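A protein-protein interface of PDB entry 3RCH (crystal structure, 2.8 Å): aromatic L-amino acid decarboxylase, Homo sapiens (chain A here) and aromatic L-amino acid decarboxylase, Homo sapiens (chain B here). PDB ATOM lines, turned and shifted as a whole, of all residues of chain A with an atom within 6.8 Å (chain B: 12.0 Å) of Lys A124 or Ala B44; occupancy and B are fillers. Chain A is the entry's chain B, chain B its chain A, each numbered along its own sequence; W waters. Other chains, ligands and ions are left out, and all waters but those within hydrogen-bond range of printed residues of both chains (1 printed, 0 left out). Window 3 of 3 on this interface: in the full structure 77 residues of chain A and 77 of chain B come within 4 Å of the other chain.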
ATOM      1  N   VAL A 117      18.948  20.727   0.305  1.00  0.00           N
ATOM      2  CA  VAL A 117      17.627  21.359   0.081  1.00  0.00           C
ATOM      3  C   VAL A 117      16.981  20.977  -1.253  1.00  0.00           C
ATOM      4  O   VAL A 117      15.766  20.809  -1.338  1.00  0.00           O
ATOM      5  CB  VAL A 117      17.701  22.884   0.189  1.00  0.00           C
ATOM      6  CG1 VAL A 117      16.359  23.482  -0.056  1.00  0.00           C
ATOM      7  CG2 VAL A 117      18.208  23.271   1.561  1.00  0.00           C
ATOM      8  N   MET A 118      17.809  20.822  -2.280  1.00  0.00           N
ATOM      9  CA  MET A 118      17.330  20.400  -3.573  1.00  0.00           C
ATOM     10  C   MET A 118      16.826  18.981  -3.506  1.00  0.00           C
ATOM     11  O   MET A 118      15.781  18.674  -4.069  1.00  0.00           O
ATOM     12  CB  MET A 118      18.411  20.541  -4.639  1.00  0.00           C
ATOM     13  CG  MET A 118      18.750  21.971  -5.023  1.00  0.00           C
ATOM     14  SD  MET A 118      17.301  22.957  -5.374  1.00  0.00           S
ATOM     15  CE  MET A 118      16.940  23.796  -3.835  1.00  0.00           C
ATOM     16  N   MET A 119      17.543  18.118  -2.797  1.00  0.00           N
ATOM     17  CA  MET A 119      17.071  16.738  -2.601  1.00  0.00           C
ATOM     18  C   MET A 119      15.719  16.699  -1.901  1.00  0.00           C
ATOM     19  O   MET A 119      14.892  15.828  -2.182  1.00  0.00           O
ATOM     20  CB  MET A 119      18.095  15.890  -1.854  1.00  0.00           C
ATOM     21  CG  MET A 119      19.334  15.552  -2.671  1.00  0.00           C
ATOM     22  SD  MET A 119      18.930  14.675  -4.200  1.00  0.00           S
ATOM     23  CE  MET A 119      18.184  13.195  -3.501  1.00  0.00           C
ATOM     24  N   ASP A 120      15.485  17.650  -1.006  1.00  0.00           N
ATOM     25  CA  ASP A 120      14.197  17.753  -0.386  1.00  0.00           C
ATOM     26  C   ASP A 120      13.147  18.181  -1.387  1.00  0.00           C
ATOM     27  O   ASP A 120      12.052  17.621  -1.414  1.00  0.00           O
ATOM     28  CB  ASP A 120      14.241  18.712   0.789  1.00  0.00           C
ATOM     29  CG  ASP A 120      14.732  18.048   2.061  1.00  0.00           C
ATOM     30  OD1 ASP A 120      14.558  16.809   2.201  1.00  0.00           O
ATOM     31  OD2 ASP A 120      15.292  18.771   2.925  1.00  0.00           O
ATOM     32  N   TRP A 121      13.478  19.174  -2.205  1.00  0.00           N
ATOM     33  CA  TRP A 121      12.557  19.660  -3.219  1.00  0.00           C
ATOM     34  C   TRP A 121      12.110  18.522  -4.120  1.00  0.00           C
ATOM     35  O   TRP A 121      10.925  18.303  -4.327  1.00  0.00           O
ATOM     36  CB  TRP A 121      13.223  20.742  -4.069  1.00  0.00           C
ATOM     37  CG  TRP A 121      13.072  22.103  -3.513  1.00  0.00           C
ATOM     38  CD1 TRP A 121      12.730  22.430  -2.231  1.00  0.00           C
ATOM     39  CD2 TRP A 121      13.287  23.342  -4.198  1.00  0.00           C
ATOM     40  NE1 TRP A 121      12.713  23.791  -2.082  1.00  0.00           N
ATOM     41  CE2 TRP A 121      13.044  24.376  -3.276  1.00  0.00           C
ATOM     42  CE3 TRP A 121      13.652  23.679  -5.507  1.00  0.00           C
ATOM     43  CZ2 TRP A 121      13.154  25.722  -3.619  1.00  0.00           C
ATOM     44  CZ3 TRP A 121      13.762  25.020  -5.843  1.00  0.00           C
ATOM     45  CH2 TRP A 121      13.510  26.018  -4.909  1.00  0.00           C
ATOM     46  N   LEU A 122      13.082  17.803  -4.660  1.00  0.00           N
ATOM     47  CA  LEU A 122      12.813  16.739  -5.594  1.00  0.00           C
ATOM     48  C   LEU A 122      11.928  15.765  -4.884  1.00  0.00           C
ATOM     49  O   LEU A 122      10.906  15.342  -5.410  1.00  0.00           O
ATOM     50  CB  LEU A 122      14.117  16.068  -5.969  1.00  0.00           C
ATOM     51  CG  LEU A 122      14.217  15.415  -7.337  1.00  0.00           C
ATOM     52  CD1 LEU A 122      13.302  16.088  -8.360  1.00  0.00           C
ATOM     53  CD2 LEU A 122      15.663  15.471  -7.784  1.00  0.00           C
ATOM     54  N   GLY A 123      12.321  15.444  -3.662  1.00  0.00           N
ATOM     55  CA  GLY A 123      11.592  14.532  -2.835  1.00  0.00           C
ATOM     56  C   GLY A 123      10.128  14.851  -2.766  1.00  0.00           C
ATOM     57  O   GLY A 123       9.310  13.986  -3.041  1.00  0.00           O
ATOM     58  N   LYS A 124       9.782  16.080  -2.392  1.00  0.00           N
ATOM     59  CA  LYS A 124       8.358  16.442  -2.255  1.00  0.00           C
ATOM     60  C   LYS A 124       7.627  16.371  -3.587  1.00  0.00           C
ATOM     61  O   LYS A 124       6.472  15.982  -3.641  1.00  0.00           O
ATOM     62  CB  LYS A 124       8.172  17.822  -1.657  1.00  0.00           C
ATOM     63  CG  LYS A 124       8.908  18.029  -0.375  1.00  0.00           C
ATOM     64  CD  LYS A 124       8.446  19.304   0.318  1.00  0.00           C
ATOM     65  CE  LYS A 124       9.364  19.587   1.481  1.00  0.00           C
ATOM     66  NZ  LYS A 124       8.903  20.760   2.259  1.00  0.00           N
ATOM     67  N   MET A 125       8.318  16.759  -4.651  1.00  0.00           N
ATOM     68  CA  MET A 125       7.800  16.674  -5.997  1.00  0.00           C
ATOM     69  C   MET A 125       7.341  15.255  -6.345  1.00  0.00           C
ATOM     70  O   MET A 125       6.275  15.058  -6.922  1.00  0.00           O
ATOM     71  CB  MET A 125       8.876  17.121  -6.970  1.00  0.00           C
ATOM     72  CG  MET A 125       8.739  18.542  -7.423  1.00  0.00           C
ATOM     73  SD  MET A 125       9.980  18.919  -8.680  1.00  0.00           S
ATOM     74  CE  MET A 125      11.232  19.652  -7.648  1.00  0.00           C
ATOM     75  N   LEU A 126       8.150  14.265  -5.994  1.00  0.00           N
ATOM     76  CA  LEU A 126       7.805  12.887  -6.257  1.00  0.00           C
ATOM     77  C   LEU A 126       6.816  12.354  -5.210  1.00  0.00           C
ATOM     78  O   LEU A 126       6.135  11.345  -5.426  1.00  0.00           O
ATOM     79  CB  LEU A 126       9.067  12.042  -6.281  1.00  0.00           C
ATOM     80  CG  LEU A 126      10.152  12.445  -7.275  1.00  0.00           C
ATOM     81  CD1 LEU A 126      11.441  11.819  -6.847  1.00  0.00           C
ATOM     82  CD2 LEU A 126       9.825  12.009  -8.651  1.00  0.00           C
ATOM     83  N   GLU A 127       6.717  13.040  -4.079  1.00  0.00           N
ATOM     84  CA  GLU A 127       5.826  12.580  -3.023  1.00  0.00           C
ATOM     85  C   GLU A 127       6.196  11.157  -2.619  1.00  0.00           C
ATOM     86  O   GLU A 127       5.376  10.239  -2.718  1.00  0.00           O
ATOM     87  CB  GLU A 127       4.365  12.655  -3.476  1.00  0.00           C
ATOM     88  CG  GLU A 127       3.881  14.078  -3.710  1.00  0.00           C
ATOM     89  CD  GLU A 127       2.604  14.343  -2.989  1.00  0.00           C
ATOM     90  OE1 GLU A 127       1.633  13.640  -3.310  1.00  0.00           O
ATOM     91  OE2 GLU A 127       2.569  15.215  -2.090  1.00  0.00           O
ATOM     92  N   LEU A 128       7.463  10.994  -2.222  1.00  0.00           N
ATOM     93  CA  LEU A 128       7.969   9.786  -1.596  1.00  0.00           C
ATOM     94  C   LEU A 128       7.381   9.776  -0.203  1.00  0.00           C
ATOM     95  O   LEU A 128       6.950  10.815   0.289  1.00  0.00           O
ATOM     96  CB  LEU A 128       9.485   9.832  -1.515  1.00  0.00           C
ATOM     97  CG  LEU A 128      10.189  10.207  -2.815  1.00  0.00           C
ATOM     98  CD1 LEU A 128      11.696  10.206  -2.657  1.00  0.00           C
ATOM     99  CD2 LEU A 128       9.798   9.260  -3.906  1.00  0.00           C
ATOM    100  N   LEU A 133      12.583  11.418   3.383  1.00  0.00           N
ATOM    101  CA  LEU A 133      12.961  12.816   3.499  1.00  0.00           C
ATOM    102  C   LEU A 133      14.114  13.043   4.465  1.00  0.00           C
ATOM    103  O   LEU A 133      14.196  12.421   5.524  1.00  0.00           O
ATOM    104  CB  LEU A 133      11.754  13.659   3.921  1.00  0.00           C
ATOM    105  CG  LEU A 133      10.553  13.646   2.975  1.00  0.00           C
ATOM    106  CD1 LEU A 133      10.065  12.223   2.747  1.00  0.00           C
ATOM    107  CD2 LEU A 133       9.432  14.521   3.515  1.00  0.00           C
ATOM    108  N   GLU A 135      14.453  16.003   5.478  1.00  0.00           N
ATOM    109  CA  GLU A 135      13.952  17.272   5.983  1.00  0.00           C
ATOM    110  C   GLU A 135      13.628  17.274   7.475  1.00  0.00           C
ATOM    111  O   GLU A 135      12.469  17.347   7.881  1.00  0.00           O
ATOM    112  CB  GLU A 135      12.720  17.710   5.187  1.00  0.00           C
ATOM    113  CG  GLU A 135      12.123  19.031   5.643  1.00  0.00           C
ATOM    114  CD  GLU A 135      10.908  19.433   4.831  1.00  0.00           C
ATOM    115  OE1 GLU A 135      10.531  18.679   3.908  1.00  0.00           O
ATOM    116  OE2 GLU A 135      10.329  20.504   5.113  1.00  0.00           O
ATOM    117  N   ILE A 280       6.282  13.173 -10.920  1.00  0.00           N
ATOM    118  CA  ILE A 280       5.884  14.492 -10.440  1.00  0.00           C
ATOM    119  C   ILE A 280       4.519  14.821 -10.953  1.00  0.00           C
ATOM    120  O   ILE A 280       3.921  15.806 -10.538  1.00  0.00           O
ATOM    121  CB  ILE A 280       6.835  15.640 -10.786  1.00  0.00           C
ATOM    122  CG1 ILE A 280       7.055  15.752 -12.281  1.00  0.00           C
ATOM    123  CG2 ILE A 280       8.121  15.543  -9.997  1.00  0.00           C
ATOM    124  CD1 ILE A 280       7.438  17.126 -12.668  1.00  0.00           C
ATOM    125  N   ARG A 285       1.780   8.573 -10.615  1.00  0.00           N
ATOM    126  CA  ARG A 285       2.187   8.208  -9.272  1.00  0.00           C
ATOM    127  C   ARG A 285       1.790   6.809  -8.848  1.00  0.00           C
ATOM    128  O   ARG A 285       2.350   6.276  -7.907  1.00  0.00           O
ATOM    129  CB  ARG A 285       1.703   9.234  -8.259  1.00  0.00           C
ATOM    130  CG  ARG A 285       2.754  10.241  -7.969  1.00  0.00           C
ATOM    131  CD  ARG A 285       2.293  11.269  -6.956  1.00  0.00           C
ATOM    132  NE  ARG A 285       2.859  12.583  -7.284  1.00  0.00           N
ATOM    133  CZ  ARG A 285       2.127  13.658  -7.572  1.00  0.00           C
ATOM    134  NH1 ARG A 285       0.797  13.593  -7.544  1.00  0.00           N
ATOM    135  NH2 ARG A 285       2.726  14.806  -7.870  1.00  0.00           N
ATOM    136  N   TRP A 315      17.643   7.908  -2.349  1.00  0.00           N
ATOM    137  CA  TRP A 315      17.179   8.078  -0.980  1.00  0.00           C
ATOM    138  C   TRP A 315      17.222   6.749  -0.277  1.00  0.00           C
ATOM    139  O   TRP A 315      16.962   5.726  -0.893  1.00  0.00           O
ATOM    140  CB  TRP A 315      15.711   8.511  -0.972  1.00  0.00           C
ATOM    141  CG  TRP A 315      15.470   9.907  -1.394  1.00  0.00           C
ATOM    142  CD1 TRP A 315      15.306  10.994  -0.577  1.00  0.00           C
ATOM    143  CD2 TRP A 315      15.357  10.391  -2.735  1.00  0.00           C
ATOM    144  NE1 TRP A 315      15.109  12.122  -1.329  1.00  0.00           N
ATOM    145  CE2 TRP A 315      15.128  11.782  -2.658  1.00  0.00           C
ATOM    146  CE3 TRP A 315      15.437   9.790  -3.995  1.00  0.00           C
ATOM    147  CZ2 TRP A 315      14.964  12.579  -3.794  1.00  0.00           C
ATOM    148  CZ3 TRP A 315      15.284  10.587  -5.126  1.00  0.00           C
ATOM    149  CH2 TRP A 315      15.053  11.965  -5.017  1.00  0.00           C
ATOM    150  N   TYR B  37      23.319  28.086   7.271  1.00  0.00           N
ATOM    151  CA  TYR B  37      22.889  29.450   7.019  1.00  0.00           C
ATOM    152  C   TYR B  37      21.930  29.433   5.834  1.00  0.00           C
ATOM    153  O   TYR B  37      20.981  30.218   5.770  1.00  0.00           O
ATOM    154  CB  TYR B  37      24.103  30.344   6.717  1.00  0.00           C
ATOM    155  CG  TYR B  37      24.562  30.285   5.277  1.00  0.00           C
ATOM    156  CD1 TYR B  37      24.246  31.304   4.388  1.00  0.00           C
ATOM    157  CD2 TYR B  37      25.276  29.192   4.792  1.00  0.00           C
ATOM    158  CE1 TYR B  37      24.646  31.251   3.054  1.00  0.00           C
ATOM    159  CE2 TYR B  37      25.685  29.129   3.451  1.00  0.00           C
ATOM    160  CZ  TYR B  37      25.364  30.165   2.582  1.00  0.00           C
ATOM    161  OH  TYR B  37      25.761  30.123   1.250  1.00  0.00           O
ATOM    162  N   LEU B  38      22.181  28.512   4.907  1.00  0.00           N
ATOM    163  CA  LEU B  38      21.505  28.504   3.617  1.00  0.00           C
ATOM    164  C   LEU B  38      20.041  28.116   3.686  1.00  0.00           C
ATOM    165  O   LEU B  38      19.193  28.833   3.149  1.00  0.00           O
ATOM    166  CB  LEU B  38      22.228  27.591   2.638  1.00  0.00           C
ATOM    167  CG  LEU B  38      21.710  27.628   1.206  1.00  0.00           C
ATOM    168  CD1 LEU B  38      22.780  28.129   0.294  1.00  0.00           C
ATOM    169  CD2 LEU B  38      21.301  26.246   0.783  1.00  0.00           C
ATOM    170  N   ARG B  39      19.737  26.994   4.334  1.00  0.00           N
ATOM    171  CA  ARG B  39      18.367  26.491   4.312  1.00  0.00           C
ATOM    172  C   ARG B  39      17.263  27.515   4.660  1.00  0.00           C
ATOM    173  O   ARG B  39      16.288  27.606   3.941  1.00  0.00           O
ATOM    174  CB  ARG B  39      18.214  25.178   5.085  1.00  0.00           C
ATOM    175  CG  ARG B  39      16.816  24.568   4.977  1.00  0.00           C
ATOM    176  CD  ARG B  39      16.649  23.374   5.908  1.00  0.00           C
ATOM    177  NE  ARG B  39      17.435  22.229   5.457  1.00  0.00           N
ATOM    178  CZ  ARG B  39      16.959  21.250   4.691  1.00  0.00           C
ATOM    179  NH1 ARG B  39      15.685  21.247   4.289  1.00  0.00           N
ATOM    180  NH2 ARG B  39      17.765  20.263   4.322  1.00  0.00           N
ATOM    181  N   PRO B  40      17.414  28.290   5.747  1.00  0.00           N
ATOM    182  CA  PRO B  40      16.353  29.278   5.998  1.00  0.00           C
ATOM    183  C   PRO B  40      16.112  30.283   4.855  1.00  0.00           C
ATOM    184  O   PRO B  40      15.004  30.802   4.719  1.00  0.00           O
ATOM    185  CB  PRO B  40      16.825  30.009   7.271  1.00  0.00           C
ATOM    186  CG  PRO B  40      18.186  29.462   7.596  1.00  0.00           C
ATOM    187  CD  PRO B  40      18.335  28.167   6.890  1.00  0.00           C
ATOM    188  N   LEU B  41      17.138  30.531   4.041  1.00  0.00           N
ATOM    189  CA  LEU B  41      17.065  31.516   2.937  1.00  0.00           C
ATOM    190  C   LEU B  41      16.338  31.035   1.683  1.00  0.00           C
ATOM    191  O   LEU B  41      16.088  31.834   0.776  1.00  0.00           O
ATOM    192  CB  LEU B  41      18.461  31.986   2.535  1.00  0.00           C
ATOM    193  CG  LEU B  41      19.232  32.686   3.643  1.00  0.00           C
ATOM    194  CD1 LEU B  41      20.595  33.048   3.127  1.00  0.00           C
ATOM    195  CD2 LEU B  41      18.462  33.911   4.142  1.00  0.00           C
ATOM    196  N   ILE B  42      16.001  29.745   1.655  1.00  0.00           N
ATOM    197  CA  ILE B  42      15.428  29.089   0.488  1.00  0.00           C
ATOM    198  C   ILE B  42      14.132  28.414   0.902  1.00  0.00           C
ATOM    199  O   ILE B  42      14.084  27.770   1.937  1.00  0.00           O
ATOM    200  CB  ILE B  42      16.421  28.045  -0.061  1.00  0.00           C
ATOM    201  CG1 ILE B  42      17.510  28.756  -0.857  1.00  0.00           C
ATOM    202  CG2 ILE B  42      15.734  27.033  -0.919  1.00  0.00           C
ATOM    203  CD1 ILE B  42      18.603  27.868  -1.282  1.00  0.00           C
ATOM    204  N   PRO B  43      13.066  28.570   0.109  1.00  0.00           N
ATOM    205  CA  PRO B  43      11.770  28.010   0.504  1.00  0.00           C
ATOM    206  C   PRO B  43      11.755  26.493   0.710  1.00  0.00           C
ATOM    207  O   PRO B  43      12.621  25.788   0.200  1.00  0.00           O
ATOM    208  CB  PRO B  43      10.848  28.437  -0.630  1.00  0.00           C
ATOM    209  CG  PRO B  43      11.452  29.732  -1.088  1.00  0.00           C
ATOM    210  CD  PRO B  43      12.936  29.508  -1.015  1.00  0.00           C
ATOM    211  N   ALA B  44      10.781  26.020   1.482  1.00  0.00           N
ATOM    212  CA  ALA B  44      10.656  24.608   1.839  1.00  0.00           C
ATOM    213  C   ALA B  44      10.437  23.687   0.644  1.00  0.00           C
ATOM    214  O   ALA B  44      10.875  22.546   0.670  1.00  0.00           O
ATOM    215  CB  ALA B  44       9.527  24.430   2.821  1.00  0.00           C
ATOM    216  N   ALA B  45       9.733  24.183  -0.379  1.00  0.00           N
ATOM    217  CA  ALA B  45       9.453  23.435  -1.632  1.00  0.00           C
ATOM    218  C   ALA B  45       9.831  24.199  -2.917  1.00  0.00           C
ATOM    219  O   ALA B  45      10.042  25.417  -2.909  1.00  0.00           O
ATOM    220  CB  ALA B  45       7.977  23.003  -1.693  1.00  0.00           C
ATOM    221  N   ALA B  46       9.916  23.464  -4.017  1.00  0.00           N
ATOM    222  CA  ALA B  46      10.031  24.056  -5.328  1.00  0.00           C
ATOM    223  C   ALA B  46       8.844  24.980  -5.621  1.00  0.00           C
ATOM    224  O   ALA B  46       7.722  24.734  -5.161  1.00  0.00           O
ATOM    225  CB  ALA B  46      10.105  22.963  -6.359  1.00  0.00           C
ATOM    226  N   PRO B  47       9.074  26.039  -6.407  1.00  0.00           N
ATOM    227  CA  PRO B  47       7.946  26.890  -6.712  1.00  0.00           C
ATOM    228  C   PRO B  47       7.043  26.290  -7.802  1.00  0.00           C
ATOM    229  O   PRO B  47       7.529  25.645  -8.734  1.00  0.00           O
ATOM    230  CB  PRO B  47       8.616  28.181  -7.191  1.00  0.00           C
ATOM    231  CG  PRO B  47       9.933  27.764  -7.728  1.00  0.00           C
ATOM    232  CD  PRO B  47      10.286  26.439  -7.141  1.00  0.00           C
ATOM    233  N   GLN B  48       5.739  26.509  -7.688  1.00  0.00           N
ATOM    234  CA  GLN B  48       4.796  25.982  -8.671  1.00  0.00           C
ATOM    235  C   GLN B  48       4.969  26.691 -10.005  1.00  0.00           C
ATOM    236  O   GLN B  48       5.093  26.055 -11.044  1.00  0.00           O
ATOM    237  CB  GLN B  48       3.357  26.110  -8.160  1.00  0.00           C
ATOM    238  CG  GLN B  48       3.024  25.170  -7.009  1.00  0.00           C
ATOM    239  CD  GLN B  48       3.067  23.682  -7.411  1.00  0.00           C
ATOM    240  OE1 GLN B  48       2.334  23.238  -8.295  1.00  0.00           O
ATOM    241  NE2 GLN B  48       3.931  22.916  -6.748  1.00  0.00           N
ATOM    242  N   ASP B  51       9.970  31.349 -10.999  1.00  0.00           N
ATOM    243  CA  ASP B  51      10.440  32.588 -10.395  1.00  0.00           C
ATOM    244  C   ASP B  51      11.044  33.520 -11.463  1.00  0.00           C
ATOM    245  O   ASP B  51      11.351  33.111 -12.589  1.00  0.00           O
ATOM    246  CB  ASP B  51      11.496  32.284  -9.330  1.00  0.00           C
ATOM    247  CG  ASP B  51      10.932  31.541  -8.109  1.00  0.00           C
ATOM    248  OD1 ASP B  51       9.750  31.740  -7.753  1.00  0.00           O
ATOM    249  OD2 ASP B  51      11.697  30.772  -7.477  1.00  0.00           O
ATOM    250  N   ASP B  59      19.239  36.354  -5.542  1.00  0.00           N
ATOM    251  CA  ASP B  59      19.481  35.257  -4.629  1.00  0.00           C
ATOM    252  C   ASP B  59      20.861  34.636  -4.769  1.00  0.00           C
ATOM    253  O   ASP B  59      21.398  34.110  -3.796  1.00  0.00           O
ATOM    254  CB  ASP B  59      18.420  34.195  -4.806  1.00  0.00           C
ATOM    255  CG  ASP B  59      17.202  34.446  -3.950  1.00  0.00           C
ATOM    256  OD1 ASP B  59      17.235  35.351  -3.072  1.00  0.00           O
ATOM    257  OD2 ASP B  59      16.214  33.706  -4.152  1.00  0.00           O
ATOM    258  N   ILE B  63      22.718  34.803  -1.447  1.00  0.00           N
ATOM    259  CA  ILE B  63      22.685  33.487  -0.816  1.00  0.00           C
ATOM    260  C   ILE B  63      23.846  32.593  -1.173  1.00  0.00           C
ATOM    261  O   ILE B  63      24.325  31.831  -0.343  1.00  0.00           O
ATOM    262  CB  ILE B  63      21.408  32.716  -1.157  1.00  0.00           C
ATOM    263  CG1 ILE B  63      20.185  33.541  -0.812  1.00  0.00           C
ATOM    264  CG2 ILE B  63      21.379  31.390  -0.414  1.00  0.00           C
ATOM    265  CD1 ILE B  63      18.942  32.982  -1.394  1.00  0.00           C
HETATM  266  O   HOH W   1       9.373  20.859  -3.801  1.00  0.00           O
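Arg B39 touches Val A117.
Ile B42 touches Val A117 (CG2 to CG1, 3.7 Å).
CZ2 of Trp A121 touches CG2 of Ile B42, 3.96 Å away.
Ala B44 touches Trp A121.
CD of Pro B47 touches CH2 of Trp A121 (3.9 Å).
CB of Ala B46 touches CE of Met A125, 3.7 Å away.
Lys A124 touches just one residue of chain B: Ala B44 (3.1 Å).
No residue of chain B comes within 4 Å of Leu A126.
No residue of chain B comes within 4 Å of Glu A127.
No residue of chain B comes within 4 Å of Leu A128.
Leu A133 touches none of the printed residues of chain B.
No residue of chain B comes within 4 Å of Glu A135.
Of the printed residues of chain A, Ile B42 touches Val A117 (3.7 Å) and Trp A121 (3.96 Å).
Printed residues of chain A within 4 Å of Pro B43: Trp A121 (3.0 Å).
Of chain A, only Trp A121 (3.4 Å) and Lys A124 (3.1 Å) come within 4 Å of Ala B44.
Printed residues of chain A within 4 Å of Ala B45: Trp A121 (3.0 Å).
Of the printed residues of chain A, Ala B46 touches Trp A121 (3.3 Å) and Met A125 (3.7 Å).
Printed residues of chain A within 4 Å of Pro B47: Trp A121.
The nearest printed residue of chain A that does not touch Arg B39 is Glu A135 (4.4 Å).
Of the 15 printed residues of chain B, 7 touch a printed residue of chain A.
Printed residues of chain B that touch a printed residue of chain A: Arg B39, Ile B42, Pro B43, Ala B44, Ala B45, Ala B46 and Pro B47.
Hydrophobic or aromatic side chains of chain B within 4 Å of the printed part of chain A: Ile B42, Ala B44, Ala B46 and Pro B47.
Hydrophobic or aromatic side chains of chain A that line the printed part of chain B: Val A117, Trp A121 and Met A125.
Among the printed residues, Asp or Glu carboxylates within 4 Å of a Lys or Arg side-chain nitrogen of the other chain: Asp A120 with Arg B39 (2.9 Å).
Water W1 lies within hydrogen-bond range of the backbone NH of Ala B46 and the backbone carbonyl oxygen of Trp A121.
OD1 of Asp A120 sits at hydrogen-bond distance from N of Glu A135 (3.4 Å).
NZ of Lys A124 is in salt-bridge range of OE1 of Glu A135, 3.1 Å away.
The indole nitrogen of Trp A121 sits close to the backbone NH of Ala B46, 3.4 Å away.
NE1 of Trp A121 sits close to O of Ala B45, at 3.2 Å.
The backbone carbonyl oxygen of Ala B44 is in hydrogen-bond range of the side-chain amino group of Lys A124 (3.1 Å).
O of Pro B43 lies within hydrogen-bond range of NE1 of Trp A121 (3.0 Å).
The guanidinium group of Arg B39 lies within salt-bridge range of the side-chain carboxylate of Asp A120.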
